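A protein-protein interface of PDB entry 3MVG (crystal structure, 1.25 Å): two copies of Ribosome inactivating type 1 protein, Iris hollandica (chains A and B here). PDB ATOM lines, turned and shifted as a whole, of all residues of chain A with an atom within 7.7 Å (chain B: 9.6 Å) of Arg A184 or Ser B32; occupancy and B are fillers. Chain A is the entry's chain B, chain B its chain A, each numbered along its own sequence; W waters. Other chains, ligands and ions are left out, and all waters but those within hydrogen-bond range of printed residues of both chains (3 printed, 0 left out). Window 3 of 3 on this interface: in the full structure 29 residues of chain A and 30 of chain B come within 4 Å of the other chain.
No position is printed for both chains.
Of the 9 pairs that touch across the chains among the printed residues, none has its exchanged pair printed and touching as well.
Among the printed residues, pairs that only touch across the chains: Ile A177 with Asp B35 (3.7 Å) and Gln A179 with Pro B37 (3.5 Å).
The guanidinium group of Arg A13 sits close to the side-chain amide nitrogen of Gln A179, 2.9 Å away.
NH1 of Arg B239 lies within hydrogen-bond range of O of His B34.
O of Pro B37 is in hydrogen-bond range of N of Leu B247.
N of Ile A177 lies within hydrogen-bond range of O of Arg A184.
The backbone carbonyl oxygen (O) of Asn A175 sits at hydrogen-bond distance from the backbone NH (N) of Asp A186, 2.9 Å away.
Printed residues of chain B that touch a printed residue of chain A: Ser B32, Asp B35, Pro B37 and Arg B239.
Of the 17 printed residues of chain A, 6 touch a printed residue of chain B.
Printed residues of chain A that touch a printed residue of chain B: Asn A174, Asn A175, Ile A177, Gln A179, Arg A184 and Asp A186.
Along chain A the printed residues that touch a printed residue of chain B span positions 174 to 186.
Water W1 lies within hydrogen-bond range of O of Asp B35, OE1 of Gln A179 and NH2 of Arg A13.
Water W3 lies within hydrogen-bond range of OD2 of Asp B35 (2.8 Å), OD1 of Asp A186 (3.3 Å) and NE of Arg A184 (3.5 Å).
Water W2 lies within hydrogen-bond range of OE1 of Gln A179 (2.9 Å) and OG of Ser B32 (2.9 Å).
Arg A184 touches two residues of chain B.
Of chain A, only Arg A184 (3.2 Å) comes within 4 Å of Ser B32.
Of the printed residues of chain B, Asp A186 touches Asp B35 (2.6 Å) and Arg B239 (3.3 Å).
Of the printed residues of chain B, Asn A175 touches Arg B239.
Of the printed residues of chain B, Gln A179 touches Asp B35 and Pro B37.
Printed residues of chain A within 4 Å of Pro B37: Gln A179 (3.5 Å).
Leu B39 touches none of the printed residues of chain A.
Leu B247 touches none of the printed residues of chain A.
The nearest residue of chain B that does not touch Arg A184 is His B34 (6.2 Å).
The nearest residue of chain A that does not touch Ser B32 is Val A180 (4.7 Å).
O of Arg B239 lies close to ND2 of Asn A174 (3.4 Å).
The guanidinium group of Arg A184 sits at hydrogen-bond distance from the side-chain hydroxyl of Ser B32 (3.2 Å).
The side-chain carboxylate of Asp B35 is in salt-bridge range of the guanidinium group of Arg A184 (2.8 Å).
The side-chain carboxylate of Asp B35 lies close to the side-chain carboxylate of Asp A186 (2.6 Å).
The backbone carbonyl oxygen (O) of Asp B35 sits close to the side-chain amide oxygen (OE1) of Gln A179 (3.2 Å).
OD1 of Asn A175 sits at hydrogen-bond distance from NE of Arg B239, at 2.9 Å.
NH2 of Arg B239 lies within salt-bridge range of OD2 of Asp A186, 3.4 Å away.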
ATOM      1  N   THR A  11      34.684   7.875 -10.681  1.00  0.00           N
ATOM      2  CA  THR A  11      35.057   7.819  -9.265  1.00  0.00           C
ATOM      3  C   THR A  11      33.931   8.259  -8.332  1.00  0.00           C
ATOM      4  O   THR A  11      33.335   9.326  -8.506  1.00  0.00           O
ATOM      5  CB  THR A  11      36.314   8.658  -8.978  1.00  0.00           C
ATOM      6  OG1 THR A  11      37.440   8.038  -9.604  1.00  0.00           O
ATOM      7  CG2 THR A  11      36.593   8.756  -7.471  1.00  0.00           C
ATOM      8  N   ARG A  13      32.861   8.086  -3.872  1.00  0.00           N
ATOM      9  CA  ARG A  13      33.447   7.948  -2.547  1.00  0.00           C
ATOM     10  C   ARG A  13      33.844   6.492  -2.299  1.00  0.00           C
ATOM     11  O   ARG A  13      34.954   6.200  -1.829  1.00  0.00           O
ATOM     12  CB  ARG A  13      32.472   8.432  -1.471  1.00  0.00           C
ATOM     13  CG  ARG A  13      32.162   9.915  -1.524  1.00  0.00           C
ATOM     14  CD  ARG A  13      31.213  10.281  -0.395  1.00  0.00           C
ATOM     15  NE  ARG A  13      30.980  11.721  -0.280  1.00  0.00           N
ATOM     16  CZ  ARG A  13      29.899  12.358  -0.726  1.00  0.00           C
ATOM     17  NH1 ARG A  13      28.922  11.705  -1.358  1.00  0.00           N
ATOM     18  NH2 ARG A  13      29.784  13.668  -0.535  1.00  0.00           N
ATOM     19  N   ILE A 126      40.022  14.861  -7.203  1.00  0.00           N
ATOM     20  CA  ILE A 126      40.080  13.961  -8.344  1.00  0.00           C
ATOM     21  C   ILE A 126      40.527  14.678  -9.625  1.00  0.00           C
ATOM     22  O   ILE A 126      41.244  14.101 -10.438  1.00  0.00           O
ATOM     23  CB  ILE A 126      38.753  13.182  -8.509  1.00  0.00           C
ATOM     24  CG1 ILE A 126      38.472  12.362  -7.236  1.00  0.00           C
ATOM     25  CG2 ILE A 126      38.776  12.297  -9.763  1.00  0.00           C
ATOM     26  CD1 ILE A 126      39.577  11.371  -6.850  1.00  0.00           C
ATOM     27  N   ASN A 127      40.120  15.929  -9.812  1.00  0.00           N
ATOM     28  CA  ASN A 127      40.604  16.666 -10.976  1.00  0.00           C
ATOM     29  C   ASN A 127      42.124  16.906 -10.930  1.00  0.00           C
ATOM     30  O   ASN A 127      42.811  16.618 -11.905  1.00  0.00           O
ATOM     31  CB  ASN A 127      39.783  17.928 -11.241  1.00  0.00           C
ATOM     32  CG  ASN A 127      38.443  17.613 -11.867  1.00  0.00           C
ATOM     33  OD1 ASN A 127      38.337  16.714 -12.700  1.00  0.00           O
ATOM     34  ND2 ASN A 127      37.416  18.341 -11.464  1.00  0.00           N
ATOM     35  N   ASN A 174      35.135  13.464   1.353  1.00  0.00           N
ATOM     36  CA  ASN A 174      34.247  14.606   1.614  1.00  0.00           C
ATOM     37  C   ASN A 174      34.093  15.541   0.417  1.00  0.00           C
ATOM     38  O   ASN A 174      33.207  16.410   0.401  1.00  0.00           O
ATOM     39  CB  ASN A 174      34.735  15.421   2.815  1.00  0.00           C
ATOM     40  CG  ASN A 174      34.575  14.690   4.123  1.00  0.00           C
ATOM     41  OD1 ASN A 174      33.920  13.655   4.196  1.00  0.00           O
ATOM     42  ND2 ASN A 174      35.188  15.225   5.168  1.00  0.00           N
ATOM     43  N   ASN A 175      34.956  15.365  -0.576  1.00  0.00           N
ATOM     44  CA  ASN A 175      34.930  16.203  -1.755  1.00  0.00           C
ATOM     45  C   ASN A 175      34.626  15.475  -3.057  1.00  0.00           C
ATOM     46  O   ASN A 175      34.717  16.068  -4.131  1.00  0.00           O
ATOM     47  CB  ASN A 175      36.226  17.012  -1.817  1.00  0.00           C
ATOM     48  CG  ASN A 175      36.208  18.148  -0.838  1.00  0.00           C
ATOM     49  OD1 ASN A 175      35.421  19.085  -0.981  1.00  0.00           O
ATOM     50  ND2 ASN A 175      37.028  18.057   0.192  1.00  0.00           N
ATOM     51  N   ILE A 176      34.259  14.198  -2.954  1.00  0.00           N
ATOM     52  CA  ILE A 176      33.736  13.448  -4.088  1.00  0.00           C
ATOM     53  C   ILE A 176      32.218  13.517  -3.951  1.00  0.00           C
ATOM     54  O   ILE A 176      31.612  12.810  -3.141  1.00  0.00           O
ATOM     55  CB  ILE A 176      34.258  11.996  -4.132  1.00  0.00           C
ATOM     56  CG1 ILE A 176      35.785  11.989  -4.293  1.00  0.00           C
ATOM     57  CG2 ILE A 176      33.567  11.218  -5.266  1.00  0.00           C
ATOM     58  CD1 ILE A 176      36.418  10.639  -4.016  1.00  0.00           C
ATOM     59  N   ILE A 177      31.612  14.424  -4.711  1.00  0.00           N
ATOM     60  CA  ILE A 177      30.205  14.773  -4.519  1.00  0.00           C
ATOM     61  C   ILE A 177      29.364  13.824  -5.375  1.00  0.00           C
ATOM     62  O   ILE A 177      28.899  14.181  -6.464  1.00  0.00           O
ATOM     63  CB  ILE A 177      29.945  16.264  -4.848  1.00  0.00           C
ATOM     64  CG1 ILE A 177      31.022  17.177  -4.223  1.00  0.00           C
ATOM     65  CG2 ILE A 177      28.528  16.673  -4.444  1.00  0.00           C
ATOM     66  CD1 ILE A 177      31.188  17.057  -2.691  1.00  0.00           C
ATOM     67  N   ASP A 178      29.199  12.598  -4.889  1.00  0.00           N
ATOM     68  CA  ASP A 178      28.598  11.550  -5.712  1.00  0.00           C
ATOM     69  C   ASP A 178      27.105  11.352  -5.442  1.00  0.00           C
ATOM     70  O   ASP A 178      26.483  10.474  -6.034  1.00  0.00           O
ATOM     71  CB  ASP A 178      29.392  10.233  -5.626  1.00  0.00           C
ATOM     72  CG  ASP A 178      29.315   9.572  -4.263  1.00  0.00           C
ATOM     73  OD1 ASP A 178      30.131   8.659  -4.023  1.00  0.00           O
ATOM     74  OD2 ASP A 178      28.446   9.922  -3.437  1.00  0.00           O
ATOM     75  N   GLN A 179      26.529  12.190  -4.585  1.00  0.00           N
ATOM     76  CA  GLN A 179      25.087  12.153  -4.331  1.00  0.00           C
ATOM     77  C   GLN A 179      24.314  12.877  -5.436  1.00  0.00           C
ATOM     78  O   GLN A 179      23.079  12.846  -5.452  1.00  0.00           O
ATOM     79  CB  GLN A 179      24.756  12.740  -2.949  1.00  0.00           C
ATOM     80  CG  GLN A 179      24.887  14.263  -2.824  1.00  0.00           C
ATOM     81  CD  GLN A 179      26.220  14.754  -2.274  1.00  0.00           C
ATOM     82  OE1 GLN A 179      26.313  15.902  -1.812  1.00  0.00           O
ATOM     83  NE2 GLN A 179      27.231  13.917  -2.312  1.00  0.00           N
ATOM     84  N   VAL A 180      25.041  13.524  -6.341  1.00  0.00           N
ATOM     85  CA  VAL A 180      24.469  14.182  -7.513  1.00  0.00           C
ATOM     86  C   VAL A 180      25.006  13.496  -8.771  1.00  0.00           C
ATOM     87  O   VAL A 180      26.034  12.806  -8.730  1.00  0.00           O
ATOM     88  CB  VAL A 180      24.791  15.696  -7.553  1.00  0.00           C
ATOM     89  CG1 VAL A 180      24.171  16.408  -6.345  1.00  0.00           C
ATOM     90  CG2 VAL A 180      26.300  15.935  -7.614  1.00  0.00           C
ATOM     91  N   THR A 181      24.313  13.710  -9.887  1.00  0.00           N
ATOM     92  CA  THR A 181      24.701  13.138 -11.175  1.00  0.00           C
ATOM     93  C   THR A 181      24.549  14.217 -12.251  1.00  0.00           C
ATOM     94  O   THR A 181      23.474  14.798 -12.396  1.00  0.00           O
ATOM     95  CB  THR A 181      23.846  11.901 -11.545  1.00  0.00           C
ATOM     96  OG1 THR A 181      23.752  11.005 -10.435  1.00  0.00           O
ATOM     97  CG2 THR A 181      24.463  11.146 -12.704  1.00  0.00           C
ATOM     98  N   PRO A 182      25.632  14.512 -12.996  1.00  0.00           N
ATOM     99  CA  PRO A 182      26.967  13.904 -12.897  1.00  0.00           C
ATOM    100  C   PRO A 182      27.638  14.159 -11.556  1.00  0.00           C
ATOM    101  O   PRO A 182      27.390  15.176 -10.908  1.00  0.00           O
ATOM    102  CB  PRO A 182      27.758  14.598 -14.012  1.00  0.00           C
ATOM    103  CG  PRO A 182      26.714  15.117 -14.958  1.00  0.00           C
ATOM    104  CD  PRO A 182      25.563  15.505 -14.082  1.00  0.00           C
ATOM    105  N   ILE A 183      28.489  13.225 -11.159  1.00  0.00           N
ATOM    106  CA  ILE A 183      29.293  13.383  -9.955  1.00  0.00           C
ATOM    107  C   ILE A 183      30.132  14.658 -10.086  1.00  0.00           C
ATOM    108  O   ILE A 183      30.663  14.950 -11.162  1.00  0.00           O
ATOM    109  CB  ILE A 183      30.204  12.154  -9.761  1.00  0.00           C
ATOM    110  CG1 ILE A 183      29.359  10.884  -9.612  1.00  0.00           C
ATOM    111  CG2 ILE A 183      31.116  12.344  -8.556  1.00  0.00           C
ATOM    112  CD1 ILE A 183      30.142   9.587  -9.783  1.00  0.00           C
ATOM    113  N   ARG A 184      30.247  15.416  -9.000  1.00  0.00           N
ATOM    114  CA  ARG A 184      31.097  16.601  -8.971  1.00  0.00           C
ATOM    115  C   ARG A 184      32.308  16.342  -8.080  1.00  0.00           C
ATOM    116  O   ARG A 184      32.234  15.561  -7.132  1.00  0.00           O
ATOM    117  CB  ARG A 184      30.300  17.831  -8.521  1.00  0.00           C
ATOM    118  CG  ARG A 184      29.080  18.116  -9.421  1.00  0.00           C
ATOM    119  CD  ARG A 184      28.486  19.501  -9.254  1.00  0.00           C
ATOM    120  NE  ARG A 184      27.763  19.694  -8.000  1.00  0.00           N
ATOM    121  CZ  ARG A 184      26.445  19.562  -7.840  1.00  0.00           C
ATOM    122  NH1 ARG A 184      25.658  19.192  -8.850  1.00  0.00           N
ATOM    123  NH2 ARG A 184      25.907  19.795  -6.649  1.00  0.00           N
ATOM    124  N   TYR A 185      33.418  16.993  -8.402  1.00  0.00           N
ATOM    125  CA  TYR A 185      34.678  16.779  -7.707  1.00  0.00           C
ATOM    126  C   TYR A 185      35.221  18.103  -7.220  1.00  0.00           C
ATOM    127  O   TYR A 185      35.568  18.971  -8.023  1.00  0.00           O
ATOM    128  CB  TYR A 185      35.674  16.094  -8.643  1.00  0.00           C
ATOM    129  CG  TYR A 185      35.178  14.757  -9.143  1.00  0.00           C
ATOM    130  CD1 TYR A 185      34.636  14.614 -10.422  1.00  0.00           C
ATOM    131  CD2 TYR A 185      35.221  13.634  -8.329  1.00  0.00           C
ATOM    132  CE1 TYR A 185      34.166  13.377 -10.872  1.00  0.00           C
ATOM    133  CE2 TYR A 185      34.767  12.401  -8.768  1.00  0.00           C
ATOM    134  CZ  TYR A 185      34.232  12.278 -10.036  1.00  0.00           C
ATOM    135  OH  TYR A 185      33.778  11.053 -10.461  1.00  0.00           O
ATOM    136  N   ASP A 186      35.283  18.278  -5.908  1.00  0.00           N
ATOM    137  CA  ASP A 186      35.790  19.515  -5.333  1.00  0.00           C
ATOM    138  C   ASP A 186      37.208  19.320  -4.827  1.00  0.00           C
ATOM    139  O   ASP A 186      37.677  18.185  -4.680  1.00  0.00           O
ATOM    140  CB  ASP A 186      34.891  19.989  -4.193  1.00  0.00           C
ATOM    141  CG  ASP A 186      33.519  20.406  -4.664  1.00  0.00           C
ATOM    142  OD1 ASP A 186      33.348  20.791  -5.840  1.00  0.00           O
ATOM    143  OD2 ASP A 186      32.596  20.360  -3.831  1.00  0.00           O
ATOM    144  N   SER B  28      17.712  13.782   2.404  1.00  0.00           N
ATOM    145  CA  SER B  28      17.904  14.967   1.591  1.00  0.00           C
ATOM    146  C   SER B  28      16.649  15.395   0.833  1.00  0.00           C
ATOM    147  O   SER B  28      15.872  14.568   0.370  1.00  0.00           O
ATOM    148  CB  SER B  28      19.003  14.666   0.584  1.00  0.00           C
ATOM    149  OG  SER B  28      19.174  15.759  -0.298  1.00  0.00           O
ATOM    150  N   SER B  29      16.485  16.709   0.696  1.00  0.00           N
ATOM    151  CA  SER B  29      15.447  17.275  -0.168  1.00  0.00           C
ATOM    152  C   SER B  29      15.821  17.213  -1.638  1.00  0.00           C
ATOM    153  O   SER B  29      15.003  17.544  -2.486  1.00  0.00           O
ATOM    154  CB  SER B  29      15.199  18.737   0.190  1.00  0.00           C
ATOM    155  OG  SER B  29      16.254  19.559  -0.288  1.00  0.00           O
ATOM    156  N   GLY B  30      17.067  16.858  -1.939  1.00  0.00           N
ATOM    157  CA  GLY B  30      17.548  16.897  -3.321  1.00  0.00           C
ATOM    158  C   GLY B  30      18.285  18.180  -3.650  1.00  0.00           C
ATOM    159  O   GLY B  30      19.208  18.176  -4.474  1.00  0.00           O
ATOM    160  N   THR B  31      17.878  19.288  -3.031  1.00  0.00           N
ATOM    161  CA  THR B  31      18.587  20.561  -3.167  1.00  0.00           C
ATOM    162  C   THR B  31      19.985  20.435  -2.567  1.00  0.00           C
ATOM    163  O   THR B  31      20.175  19.828  -1.507  1.00  0.00           O
ATOM    164  CB  THR B  31      17.802  21.710  -2.505  1.00  0.00           C
ATOM    165  OG1 THR B  31      16.532  21.837  -3.155  1.00  0.00           O
ATOM    166  CG2 THR B  31      18.544  23.046  -2.603  1.00  0.00           C
ATOM    167  N   SER B  32      20.951  21.005  -3.280  1.00  0.00           N
ATOM    168  CA  SER B  32      22.358  20.985  -2.920  1.00  0.00           C
ATOM    169  C   SER B  32      22.785  22.424  -2.660  1.00  0.00           C
ATOM    170  O   SER B  32      22.490  23.311  -3.472  1.00  0.00           O
ATOM    171  CB  SER B  32      23.157  20.418  -4.098  1.00  0.00           C
ATOM    172  OG  SER B  32      24.538  20.297  -3.803  1.00  0.00           O
ATOM    173  N   VAL B  33      23.449  22.668  -1.533  1.00  0.00           N
ATOM    174  CA  VAL B  33      24.012  23.995  -1.241  1.00  0.00           C
ATOM    175  C   VAL B  33      25.503  23.816  -0.972  1.00  0.00           C
ATOM    176  O   VAL B  33      25.890  23.116  -0.027  1.00  0.00           O
ATOM    177  CB  VAL B  33      23.312  24.682  -0.036  1.00  0.00           C
ATOM    178  CG1 VAL B  33      23.945  26.038   0.251  1.00  0.00           C
ATOM    179  CG2 VAL B  33      21.811  24.858  -0.301  1.00  0.00           C
ATOM    180  N   HIS B  34      26.339  24.422  -1.815  1.00  0.00           N
ATOM    181  CA  HIS B  34      27.796  24.224  -1.744  1.00  0.00           C
ATOM    182  C   HIS B  34      28.179  22.746  -1.655  1.00  0.00           C
ATOM    183  O   HIS B  34      29.069  22.359  -0.890  1.00  0.00           O
ATOM    184  CB  HIS B  34      28.411  25.006  -0.585  1.00  0.00           C
ATOM    185  CG  HIS B  34      28.283  26.488  -0.730  1.00  0.00           C
ATOM    186  ND1 HIS B  34      29.043  27.208  -1.627  1.00  0.00           N
ATOM    187  CD2 HIS B  34      27.487  27.383  -0.099  1.00  0.00           C
ATOM    188  CE1 HIS B  34      28.720  28.487  -1.538  1.00  0.00           C
ATOM    189  NE2 HIS B  34      27.776  28.620  -0.624  1.00  0.00           N
ATOM    190  N   ASP B  35      27.475  21.930  -2.439  1.00  0.00           N
ATOM    191  CA  ASP B  35      27.733  20.489  -2.551  1.00  0.00           C
ATOM    192  C   ASP B  35      27.425  19.690  -1.285  1.00  0.00           C
ATOM    193  O   ASP B  35      27.936  18.576  -1.112  1.00  0.00           O
ATOM    194  CB  ASP B  35      29.136  20.206  -3.101  1.00  0.00           C
ATOM    195  CG  ASP B  35      29.279  20.642  -4.536  1.00  0.00           C
ATOM    196  OD1 ASP B  35      28.276  20.594  -5.281  1.00  0.00           O
ATOM    197  OD2 ASP B  35      30.391  21.039  -4.922  1.00  0.00           O
ATOM    198  N   ILE B  36      26.597  20.270  -0.418  1.00  0.00           N
ATOM    199  CA  ILE B  36      26.067  19.581   0.747  1.00  0.00           C
ATOM    200  C   ILE B  36      24.544  19.518   0.598  1.00  0.00           C
ATOM    201  O   ILE B  36      23.911  20.524   0.256  1.00  0.00           O
ATOM    202  CB  ILE B  36      26.441  20.290   2.067  1.00  0.00           C
ATOM    203  CG1 ILE B  36      27.939  20.610   2.106  1.00  0.00           C
ATOM    204  CG2 ILE B  36      26.031  19.435   3.268  1.00  0.00           C
ATOM    205  CD1 ILE B  36      28.355  21.389   3.323  1.00  0.00           C
ATOM    206  N   PRO B  37      23.948  18.335   0.826  1.00  0.00           N
ATOM    207  CA  PRO B  37      22.490  18.230   0.735  1.00  0.00           C
ATOM    208  C   PRO B  37      21.760  19.111   1.740  1.00  0.00           C
ATOM    209  O   PRO B  37      22.139  19.185   2.915  1.00  0.00           O
ATOM    210  CB  PRO B  37      22.224  16.762   1.069  1.00  0.00           C
ATOM    211  CG  PRO B  37      23.461  16.062   0.654  1.00  0.00           C
ATOM    212  CD  PRO B  37      24.575  17.008   0.996  1.00  0.00           C
ATOM    213  N   LEU B  38      20.708  19.761   1.260  1.00  0.00           N
ATOM    214  CA  LEU B  38      19.832  20.562   2.094  1.00  0.00           C
ATOM    215  C   LEU B  38      18.650  19.712   2.521  1.00  0.00           C
ATOM    216  O   LEU B  38      17.988  19.095   1.684  1.00  0.00           O
ATOM    217  CB  LEU B  38      19.338  21.767   1.294  1.00  0.00           C
ATOM    218  CG  LEU B  38      18.495  22.824   2.016  1.00  0.00           C
ATOM    219  CD1 LEU B  38      19.301  23.509   3.097  1.00  0.00           C
ATOM    220  CD2 LEU B  38      17.989  23.846   1.004  1.00  0.00           C
ATOM    221  N   LEU B  39      18.388  19.656   3.820  1.00  0.00           N
ATOM    222  CA  LEU B  39      17.243  18.902   4.314  1.00  0.00           C
ATOM    223  C   LEU B  39      15.941  19.629   3.960  1.00  0.00           C
ATOM    224  O   LEU B  39      15.951  20.842   3.680  1.00  0.00           O
ATOM    225  CB  LEU B  39      17.380  18.660   5.820  1.00  0.00           C
ATOM    226  CG  LEU B  39      18.518  17.696   6.193  1.00  0.00           C
ATOM    227  CD1 LEU B  39      18.653  17.609   7.687  1.00  0.00           C
ATOM    228  CD2 LEU B  39      18.318  16.288   5.598  1.00  0.00           C
ATOM    229  N   VAL B 208      26.758  27.963   6.302  1.00  0.00           N
ATOM    230  CA  VAL B 208      26.912  27.504   4.923  1.00  0.00           C
ATOM    231  C   VAL B 208      25.879  28.171   4.002  1.00  0.00           C
ATOM    232  O   VAL B 208      26.219  28.607   2.895  1.00  0.00           O
ATOM    233  CB  VAL B 208      26.880  25.961   4.818  1.00  0.00           C
ATOM    234  CG1 VAL B 208      26.749  25.503   3.360  1.00  0.00           C
ATOM    235  CG2 VAL B 208      28.116  25.374   5.452  1.00  0.00           C
ATOM    236  N   GLN B 209      24.638  28.257   4.469  1.00  0.00           N
ATOM    237  CA  GLN B 209      23.558  28.832   3.662  1.00  0.00           C
ATOM    238  C   GLN B 209      23.667  30.347   3.468  1.00  0.00           C
ATOM    239  O   GLN B 209      23.205  30.867   2.451  1.00  0.00           O
ATOM    240  CB  GLN B 209      22.183  28.440   4.208  1.00  0.00           C
ATOM    241  CG  GLN B 209      21.851  26.981   3.928  1.00  0.00           C
ATOM    242  CD  GLN B 209      20.752  26.456   4.807  1.00  0.00           C
ATOM    243  OE1 GLN B 209      19.571  26.609   4.509  1.00  0.00           O
ATOM    244  NE2 GLN B 209      21.135  25.824   5.910  1.00  0.00           N
ATOM    245  N   VAL B 235      32.874  27.585   3.670  1.00  0.00           N
ATOM    246  CA  VAL B 235      32.113  26.389   3.338  1.00  0.00           C
ATOM    247  C   VAL B 235      33.007  25.185   3.071  1.00  0.00           C
ATOM    248  O   VAL B 235      32.714  24.076   3.526  1.00  0.00           O
ATOM    249  CB  VAL B 235      31.223  26.609   2.115  1.00  0.00           C
ATOM    250  CG1 VAL B 235      30.495  25.329   1.802  1.00  0.00           C
ATOM    251  CG2 VAL B 235      30.248  27.737   2.374  1.00  0.00           C
ATOM    252  N   ARG B 239      32.758  21.536   4.853  1.00  0.00           N
ATOM    253  CA  ARG B 239      32.559  20.297   4.107  1.00  0.00           C
ATOM    254  C   ARG B 239      33.732  19.333   4.282  1.00  0.00           C
ATOM    255  O   ARG B 239      33.536  18.121   4.423  1.00  0.00           O
ATOM    256  CB  ARG B 239      32.319  20.609   2.624  1.00  0.00           C
ATOM    257  CG  ARG B 239      31.829  19.403   1.804  1.00  0.00           C
ATOM    258  CD  ARG B 239      31.572  19.753   0.332  1.00  0.00           C
ATOM    259  NE  ARG B 239      32.806  20.229  -0.273  1.00  0.00           N
ATOM    260  CZ  ARG B 239      33.013  21.456  -0.732  1.00  0.00           C
ATOM    261  NH1 ARG B 239      32.033  22.353  -0.773  1.00  0.00           N
ATOM    262  NH2 ARG B 239      34.215  21.767  -1.187  1.00  0.00           N
ATOM    263  N   ALA B 245      27.593  17.120   6.257  1.00  0.00           N
ATOM    264  CA  ALA B 245      27.081  16.242   5.208  1.00  0.00           C
ATOM    265  C   ALA B 245      25.600  16.383   4.937  1.00  0.00           C
ATOM    266  O   ALA B 245      25.093  15.824   3.968  1.00  0.00           O
ATOM    267  CB  ALA B 245      27.420  14.782   5.529  1.00  0.00           C
ATOM    268  N   LEU B 246      24.908  17.095   5.822  1.00  0.00           N
ATOM    269  CA  LEU B 246      23.497  17.448   5.674  1.00  0.00           C
ATOM    270  C   LEU B 246      23.328  18.822   6.283  1.00  0.00           C
ATOM    271  O   LEU B 246      23.956  19.116   7.305  1.00  0.00           O
ATOM    272  CB  LEU B 246      22.585  16.479   6.438  1.00  0.00           C
ATOM    273  CG  LEU B 246      22.600  15.002   6.056  1.00  0.00           C
ATOM    274  CD1 LEU B 246      21.815  14.196   7.069  1.00  0.00           C
ATOM    275  CD2 LEU B 246      22.039  14.814   4.658  1.00  0.00           C
ATOM    276  N   LEU B 247      22.475  19.643   5.679  1.00  0.00           N
ATOM    277  CA  LEU B 247      22.233  20.992   6.185  1.00  0.00           C
ATOM    278  C   LEU B 247      20.827  21.142   6.722  1.00  0.00           C
ATOM    279  O   LEU B 247      19.852  20.863   6.017  1.00  0.00           O
ATOM    280  CB  LEU B 247      22.438  22.041   5.089  1.00  0.00           C
ATOM    281  CG  LEU B 247      23.772  22.073   4.364  1.00  0.00           C
ATOM    282  CD1 LEU B 247      23.667  23.032   3.200  1.00  0.00           C
ATOM    283  CD2 LEU B 247      24.915  22.453   5.275  1.00  0.00           C
ATOM    284  N   ARG B 249      17.823  23.211   7.087  1.00  0.00           N
ATOM    285  CA  ARG B 249      17.370  24.335   6.263  1.00  0.00           C
ATOM    286  C   ARG B 249      17.124  25.567   7.128  1.00  0.00           C
ATOM    287  O   ARG B 249      16.420  25.506   8.143  1.00  0.00           O
ATOM    288  CB  ARG B 249      16.130  23.956   5.456  1.00  0.00           C
ATOM    289  CG  ARG B 249      15.690  25.024   4.446  1.00  0.00           C
ATOM    290  CD  ARG B 249      14.496  24.572   3.628  1.00  0.00           C
ATOM    291  NE  ARG B 249      14.843  23.408   2.815  1.00  0.00           N
ATOM    292  CZ  ARG B 249      14.334  23.121   1.625  1.00  0.00           C
ATOM    293  NH1 ARG B 249      13.402  23.899   1.077  1.00  0.00           N
ATOM    294  NH2 ARG B 249      14.755  22.043   0.976  1.00  0.00           N
HETATM  295  O   HOH W   1      28.346  16.427   0.520  1.00  0.00           O
HETATM  296  O   HOH W   2      24.201  17.777  -2.366  1.00  0.00           O
HETATM  297  O   HOH W   3      30.669  21.518  -7.633  1.00  0.00           O
